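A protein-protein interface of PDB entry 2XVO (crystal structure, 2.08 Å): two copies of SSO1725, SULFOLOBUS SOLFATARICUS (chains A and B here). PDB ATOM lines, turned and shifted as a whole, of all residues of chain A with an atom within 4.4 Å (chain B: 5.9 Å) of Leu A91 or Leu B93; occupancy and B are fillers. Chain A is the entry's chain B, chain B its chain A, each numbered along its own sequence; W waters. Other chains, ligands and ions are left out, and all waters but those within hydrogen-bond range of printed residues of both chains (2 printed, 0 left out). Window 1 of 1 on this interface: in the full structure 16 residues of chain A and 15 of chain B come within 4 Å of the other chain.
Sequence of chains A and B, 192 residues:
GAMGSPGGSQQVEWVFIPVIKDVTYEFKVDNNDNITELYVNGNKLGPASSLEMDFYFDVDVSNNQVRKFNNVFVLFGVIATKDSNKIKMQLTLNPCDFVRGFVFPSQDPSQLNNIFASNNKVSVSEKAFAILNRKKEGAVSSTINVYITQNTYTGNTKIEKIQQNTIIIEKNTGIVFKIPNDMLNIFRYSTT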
ATOM      1  N   LEU A  75     -19.143  -8.139  10.713  1.00  0.00           N
ATOM      2  CA  LEU A  75     -19.932  -7.136   9.996  1.00  0.00           C
ATOM      3  C   LEU A  75     -21.136  -7.814   9.342  1.00  0.00           C
ATOM      4  O   LEU A  75     -20.975  -8.793   8.612  1.00  0.00           O
ATOM      5  CB  LEU A  75     -19.067  -6.453   8.942  1.00  0.00           C
ATOM      6  CG  LEU A  75     -19.604  -5.198   8.249  1.00  0.00           C
ATOM      7  CD1 LEU A  75     -19.883  -4.054   9.231  1.00  0.00           C
ATOM      8  CD2 LEU A  75     -18.628  -4.769   7.182  1.00  0.00           C
ATOM      9  N   PHE A  76     -22.339  -7.313   9.623  1.00  0.00           N
ATOM     10  CA  PHE A  76     -23.576  -7.917   9.123  1.00  0.00           C
ATOM     11  C   PHE A  76     -24.069  -7.162   7.888  1.00  0.00           C
ATOM     12  O   PHE A  76     -23.820  -5.964   7.738  1.00  0.00           O
ATOM     13  CB  PHE A  76     -24.679  -7.926  10.213  1.00  0.00           C
ATOM     14  CG  PHE A  76     -24.332  -8.762  11.402  1.00  0.00           C
ATOM     15  CD1 PHE A  76     -24.624 -10.115  11.439  1.00  0.00           C
ATOM     16  CD2 PHE A  76     -23.655  -8.204  12.468  1.00  0.00           C
ATOM     17  CE1 PHE A  76     -24.247 -10.903  12.548  1.00  0.00           C
ATOM     18  CE2 PHE A  76     -23.291  -8.969  13.568  1.00  0.00           C
ATOM     19  CZ  PHE A  76     -23.582 -10.321  13.603  1.00  0.00           C
ATOM     20  N   GLY A  77     -24.802  -7.872   7.031  1.00  0.00           N
ATOM     21  CA  GLY A  77     -25.385  -7.269   5.834  1.00  0.00           C
ATOM     22  C   GLY A  77     -24.414  -7.214   4.663  1.00  0.00           C
ATOM     23  O   GLY A  77     -24.609  -6.459   3.740  1.00  0.00           O
ATOM     24  N   VAL A  78     -23.361  -8.027   4.722  1.00  0.00           N
ATOM     25  CA  VAL A  78     -22.338  -8.080   3.688  1.00  0.00           C
ATOM     26  C   VAL A  78     -21.916  -9.518   3.436  1.00  0.00           C
ATOM     27  O   VAL A  78     -22.104 -10.382   4.297  1.00  0.00           O
ATOM     28  CB  VAL A  78     -21.073  -7.280   4.094  1.00  0.00           C
ATOM     29  CG1 VAL A  78     -21.405  -5.803   4.276  1.00  0.00           C
ATOM     30  CG2 VAL A  78     -20.482  -7.851   5.350  1.00  0.00           C
ATOM     31  N   GLN A  90     -19.125  -7.344  -0.672  1.00  0.00           N
ATOM     32  CA  GLN A  90     -20.303  -6.718  -1.260  1.00  0.00           C
ATOM     33  C   GLN A  90     -21.400  -6.524  -0.228  1.00  0.00           C
ATOM     34  O   GLN A  90     -21.579  -7.356   0.653  1.00  0.00           O
ATOM     35  CB  GLN A  90     -20.835  -7.599  -2.392  1.00  0.00           C
ATOM     36  CG  GLN A  90     -19.995  -7.547  -3.645  1.00  0.00           C
ATOM     37  CD  GLN A  90     -20.534  -8.440  -4.697  1.00  0.00           C
ATOM     38  OE1 GLN A  90     -21.272  -8.007  -5.595  1.00  0.00           O
ATOM     39  NE2 GLN A  90     -20.224  -9.712  -4.570  1.00  0.00           N
ATOM     40  N   LEU A  91     -22.129  -5.421  -0.365  1.00  0.00           N
ATOM     41  CA  LEU A  91     -23.316  -5.130   0.447  1.00  0.00           C
ATOM     42  C   LEU A  91     -24.509  -5.981  -0.008  1.00  0.00           C
ATOM     43  O   LEU A  91     -24.781  -6.057  -1.207  1.00  0.00           O
ATOM     44  CB  LEU A  91     -23.674  -3.655   0.290  1.00  0.00           C
ATOM     45  CG  LEU A  91     -24.836  -3.080   1.118  1.00  0.00           C
ATOM     46  CD1 LEU A  91     -24.504  -3.051   2.631  1.00  0.00           C
ATOM     47  CD2 LEU A  91     -25.223  -1.712   0.555  1.00  0.00           C
ATOM     48  N   THR A  92     -25.186  -6.635   0.937  1.00  0.00           N
ATOM     49  CA  THR A  92     -26.484  -7.277   0.676  1.00  0.00           C
ATOM     50  C   THR A  92     -27.622  -6.655   1.506  1.00  0.00           C
ATOM     51  O   THR A  92     -28.787  -6.733   1.117  1.00  0.00           O
ATOM     52  CB  THR A  92     -26.468  -8.801   0.998  1.00  0.00           C
ATOM     53  OG1 THR A  92     -26.349  -8.981   2.410  1.00  0.00           O
ATOM     54  CG2 THR A  92     -25.328  -9.531   0.279  1.00  0.00           C
ATOM     55  N   LEU A  93     -27.275  -6.056   2.649  1.00  0.00           N
ATOM     56  CA  LEU A  93     -28.227  -5.523   3.625  1.00  0.00           C
ATOM     57  C   LEU A  93     -29.099  -6.595   4.259  1.00  0.00           C
ATOM     58  O   LEU A  93     -30.059  -6.278   4.960  1.00  0.00           O
ATOM     59  CB  LEU A  93     -29.075  -4.374   3.032  1.00  0.00           C
ATOM     60  CG  LEU A  93     -28.377  -3.017   2.964  1.00  0.00           C
ATOM     61  CD1 LEU A  93     -29.216  -1.989   2.245  1.00  0.00           C
ATOM     62  CD2 LEU A  93     -28.049  -2.538   4.387  1.00  0.00           C
ATOM     63  N   VAL A 124     -17.131   2.847   8.685  1.00  0.00           N
ATOM     64  CA  VAL A 124     -18.227   2.242   9.413  1.00  0.00           C
ATOM     65  C   VAL A 124     -17.954   2.400  10.893  1.00  0.00           C
ATOM     66  O   VAL A 124     -16.829   2.192  11.355  1.00  0.00           O
ATOM     67  CB  VAL A 124     -18.371   0.761   9.063  1.00  0.00           C
ATOM     68  CG1 VAL A 124     -19.464   0.078   9.939  1.00  0.00           C
ATOM     69  CG2 VAL A 124     -18.662   0.622   7.582  1.00  0.00           C
ATOM     70  N   ALA A 128     -21.025  -0.658  15.020  1.00  0.00           N
ATOM     71  CA  ALA A 128     -21.833  -1.466  14.096  1.00  0.00           C
ATOM     72  C   ALA A 128     -21.408  -2.922  14.067  1.00  0.00           C
ATOM     73  O   ALA A 128     -22.208  -3.784  13.715  1.00  0.00           O
ATOM     74  CB  ALA A 128     -21.780  -0.900  12.692  1.00  0.00           C
ATOM     75  N   ILE A 148     -15.484  -2.176   0.278  1.00  0.00           N
ATOM     76  CA  ILE A 148     -16.695  -2.778  -0.219  1.00  0.00           C
ATOM     77  C   ILE A 148     -16.909  -2.231  -1.624  1.00  0.00           C
ATOM     78  O   ILE A 148     -16.657  -1.058  -1.862  1.00  0.00           O
ATOM     79  CB  ILE A 148     -17.847  -2.428   0.748  1.00  0.00           C
ATOM     80  CG1 ILE A 148     -19.092  -3.266   0.475  1.00  0.00           C
ATOM     81  CG2 ILE A 148     -18.134  -0.925   0.710  1.00  0.00           C
ATOM     82  CD1 ILE A 148     -20.020  -3.337   1.678  1.00  0.00           C
ATOM     83  N   THR A 152     -24.246  -3.792  -5.146  1.00  0.00           N
ATOM     84  CA  THR A 152     -24.875  -4.713  -4.234  1.00  0.00           C
ATOM     85  C   THR A 152     -24.971  -6.121  -4.819  1.00  0.00           C
ATOM     86  O   THR A 152     -24.968  -6.297  -6.028  1.00  0.00           O
ATOM     87  CB  THR A 152     -26.282  -4.158  -3.922  1.00  0.00           C
ATOM     88  OG1 THR A 152     -26.911  -4.973  -2.935  1.00  0.00           O
ATOM     89  CG2 THR A 152     -27.099  -4.127  -5.143  1.00  0.00           C
ATOM     90  N   TYR A 153     -25.070  -7.117  -3.950  1.00  0.00           N
ATOM     91  CA  TYR A 153     -25.356  -8.484  -4.364  1.00  0.00           C
ATOM     92  C   TYR A 153     -26.745  -8.880  -3.866  1.00  0.00           C
ATOM     93  O   TYR A 153     -27.043  -8.779  -2.676  1.00  0.00           O
ATOM     94  CB  TYR A 153     -24.320  -9.451  -3.792  1.00  0.00           C
ATOM     95  CG  TYR A 153     -24.563 -10.874  -4.179  1.00  0.00           C
ATOM     96  CD1 TYR A 153     -24.269 -11.326  -5.466  1.00  0.00           C
ATOM     97  CD2 TYR A 153     -25.077 -11.795  -3.259  1.00  0.00           C
ATOM     98  CE1 TYR A 153     -24.504 -12.658  -5.835  1.00  0.00           C
ATOM     99  CE2 TYR A 153     -25.308 -13.120  -3.614  1.00  0.00           C
ATOM    100  CZ  TYR A 153     -25.021 -13.541  -4.902  1.00  0.00           C
ATOM    101  OH  TYR A 153     -25.244 -14.852  -5.252  1.00  0.00           O
ATOM    102  N   GLY B  77     -29.735  -1.870   9.422  1.00  0.00           N
ATOM    103  CA  GLY B  77     -28.415  -1.343   9.072  1.00  0.00           C
ATOM    104  C   GLY B  77     -28.486  -0.021   8.339  1.00  0.00           C
ATOM    105  O   GLY B  77     -27.523   0.390   7.694  1.00  0.00           O
ATOM    106  N   VAL B  78     -29.627   0.659   8.446  1.00  0.00           N
ATOM    107  CA  VAL B  78     -29.835   1.953   7.797  1.00  0.00           C
ATOM    108  C   VAL B  78     -30.575   2.900   8.731  1.00  0.00           C
ATOM    109  O   VAL B  78     -31.221   2.458   9.682  1.00  0.00           O
ATOM    110  CB  VAL B  78     -30.646   1.819   6.498  1.00  0.00           C
ATOM    111  CG1 VAL B  78     -29.872   0.964   5.454  1.00  0.00           C
ATOM    112  CG2 VAL B  78     -32.003   1.237   6.778  1.00  0.00           C
ATOM    113  N   LEU B  91     -26.669   4.411   5.001  1.00  0.00           N
ATOM    114  CA  LEU B  91     -26.132   3.140   5.473  1.00  0.00           C
ATOM    115  C   LEU B  91     -25.332   3.348   6.751  1.00  0.00           C
ATOM    116  O   LEU B  91     -24.499   4.254   6.818  1.00  0.00           O
ATOM    117  CB  LEU B  91     -25.214   2.550   4.391  1.00  0.00           C
ATOM    118  CG  LEU B  91     -24.652   1.143   4.629  1.00  0.00           C
ATOM    119  CD1 LEU B  91     -25.782   0.107   4.632  1.00  0.00           C
ATOM    120  CD2 LEU B  91     -23.610   0.798   3.580  1.00  0.00           C
ATOM    121  N   THR B  92     -25.607   2.538   7.774  1.00  0.00           N
ATOM    122  CA  THR B  92     -24.746   2.459   8.975  1.00  0.00           C
ATOM    123  C   THR B  92     -24.125   1.073   9.157  1.00  0.00           C
ATOM    124  O   THR B  92     -23.083   0.938   9.796  1.00  0.00           O
ATOM    125  CB  THR B  92     -25.521   2.800  10.269  1.00  0.00           C
ATOM    126  OG1 THR B  92     -26.479   1.774  10.545  1.00  0.00           O
ATOM    127  CG2 THR B  92     -26.243   4.152  10.145  1.00  0.00           C
ATOM    128  N   LEU B  93     -24.776   0.045   8.604  1.00  0.00           N
ATOM    129  CA  LEU B  93     -24.404  -1.370   8.799  1.00  0.00           C
ATOM    130  C   LEU B  93     -24.520  -1.831  10.263  1.00  0.00           C
ATOM    131  O   LEU B  93     -24.090  -2.924  10.604  1.00  0.00           O
ATOM    132  CB  LEU B  93     -23.027  -1.678   8.206  1.00  0.00           C
ATOM    133  CG  LEU B  93     -23.014  -1.822   6.673  1.00  0.00           C
ATOM    134  CD1 LEU B  93     -21.597  -2.036   6.135  1.00  0.00           C
ATOM    135  CD2 LEU B  93     -23.949  -2.918   6.179  1.00  0.00           C
ATOM    136  N   ASN B  94     -25.117  -0.997  11.114  1.00  0.00           N
ATOM    137  CA  ASN B  94     -25.410  -1.362  12.494  1.00  0.00           C
ATOM    138  C   ASN B  94     -26.762  -2.095  12.553  1.00  0.00           C
ATOM    139  O   ASN B  94     -27.779  -1.496  12.243  1.00  0.00           O
ATOM    140  CB  ASN B  94     -25.462  -0.082  13.358  1.00  0.00           C
ATOM    141  CG  ASN B  94     -25.522  -0.377  14.825  1.00  0.00           C
ATOM    142  OD1 ASN B  94     -25.979  -1.445  15.253  1.00  0.00           O
ATOM    143  ND2 ASN B  94     -25.007   0.548  15.615  1.00  0.00           N
ATOM    144  N   PRO B  95     -26.780  -3.373  12.970  1.00  0.00           N
ATOM    145  CA  PRO B  95     -28.029  -4.132  12.928  1.00  0.00           C
ATOM    146  C   PRO B  95     -29.095  -3.611  13.903  1.00  0.00           C
ATOM    147  O   PRO B  95     -30.273  -3.962  13.742  1.00  0.00           O
ATOM    148  CB  PRO B  95     -27.610  -5.563  13.306  1.00  0.00           C
ATOM    149  CG  PRO B  95     -26.195  -5.545  13.633  1.00  0.00           C
ATOM    150  CD  PRO B  95     -25.639  -4.173  13.461  1.00  0.00           C
ATOM    151  N   ASP B  97     -29.807  -0.472  14.052  1.00  0.00           N
ATOM    152  CA  ASP B  97     -30.497   0.544  13.258  1.00  0.00           C
ATOM    153  C   ASP B  97     -31.490  -0.090  12.290  1.00  0.00           C
ATOM    154  O   ASP B  97     -31.203  -1.119  11.691  1.00  0.00           O
ATOM    155  CB  ASP B  97     -29.498   1.379  12.435  1.00  0.00           C
ATOM    156  CG  ASP B  97     -28.596   2.251  13.295  1.00  0.00           C
ATOM    157  OD1 ASP B  97     -28.988   2.603  14.427  1.00  0.00           O
ATOM    158  OD2 ASP B  97     -27.495   2.592  12.829  1.00  0.00           O
ATOM    159  N   VAL B 122     -29.940   1.520  -5.017  1.00  0.00           N
ATOM    160  CA  VAL B 122     -29.379   0.197  -5.187  1.00  0.00           C
ATOM    161  C   VAL B 122     -30.498  -0.826  -5.107  1.00  0.00           C
ATOM    162  O   VAL B 122     -31.520  -0.594  -4.434  1.00  0.00           O
ATOM    163  CB  VAL B 122     -28.300  -0.121  -4.107  1.00  0.00           C
ATOM    164  CG1 VAL B 122     -27.038   0.757  -4.300  1.00  0.00           C
ATOM    165  CG2 VAL B 122     -28.868   0.047  -2.704  1.00  0.00           C
HETATM  166  O   HOH W   1     -25.868  -4.590   8.947  1.00  0.00           O
HETATM  167  O   HOH W   2     -22.613  -5.081  11.400  1.00  0.00           O
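Water W2 lies within hydrogen-bond range of O of Ala A128 (2.7 Å), O of Leu B93 (2.7 Å) and N of Phe A76 (2.9 Å).
Water W1 bridges the backbone carbonyl oxygen of Phe A76 (2.7 Å) and the backbone carbonyl oxygen of Leu B93 (2.9 Å).
The backbone carbonyl oxygen (O) of Gly B77 is in hydrogen-bond range of the backbone NH (N) of Thr B92, 2.9 Å away.
O of Gly B77 is in hydrogen-bond range of N of Leu B93 (2.9 Å).
The backbone carbonyl oxygen (O) of Asn B94 lies close to the backbone NH (N) of Gly B77.
The side-chain hydroxyl (OG1) of Thr B92 lies within hydrogen-bond range of the side-chain carboxylate (OD2) of Asp B97, 2.6 Å away.
O of Gly A77 is in hydrogen-bond range of N of Leu A93, at 2.9 Å.
The backbone carbonyl oxygen (O) of Leu A91 sits at hydrogen-bond distance from the side-chain hydroxyl (OG1) of Thr A152.
Leu B91 touches its own counterpart, Leu A91.
Leu A91 touches Leu B93, and with the chains exchanged Leu A93 touches Leu B91.
Leu A91 touches just these residues of chain B: Leu B91 and Leu B93.
Of chain A, only Phe A76, Leu A91 and Ala A128 come within 4 Å of Leu B93.
Of the printed residues of chain A, Leu B91 touches Leu A91 and Leu A93.
Printed residues of chain A within 4 Å of Pro B95: Phe A76 (3.9 Å) and Ala A128 (3.5 Å).
Tyr A153 touches none of the printed residues of chain B.
Val A78 touches none of the printed residues of chain B.
The nearest residue of chain B that does not touch Leu A91 is Val B122 (5.2 Å).
The nearest residue of chain A that does not touch Leu B93 is Leu A75 (4.1 Å).
The nearest printed residue of chain B that does not touch Leu A93 is Val B78 (4.1 Å).
Phe A76 touches Leu B93 (O to CD2, 3.4 Å).
Phe A76 touches Pro B95 (CD2 to CG, 3.9 Å).
Leu A91 touches Leu B91.
CD1 of Leu A91 touches CD2 of Leu B93, 3.6 Å away.
Leu B91 touches Leu A93.
Thr B92 touches Val A124 (O to CG1, 3.7 Å).
Thr B92 touches Ala A128 (O to CB, 3.7 Å).
Ala A128 touches Leu B93.
CB of Ala A128 touches CA of Asn B94 (3.7 Å).
Ala A128 touches Pro B95 (O to CD, 3.5 Å).
Hydrophobic or aromatic side chains of chain B that line the printed part of chain A: Leu B91, Leu B93 and Pro B95.
Of the 13 printed residues of chain A, 5 touch a printed residue of chain B.
Hydrophobic or aromatic side chains of chain A within 4 Å of the printed part of chain B: Phe A76, Leu A91, Leu A93, Val A124 and Ala A128.
Among the printed residues, 10 pairs touch across the chains.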
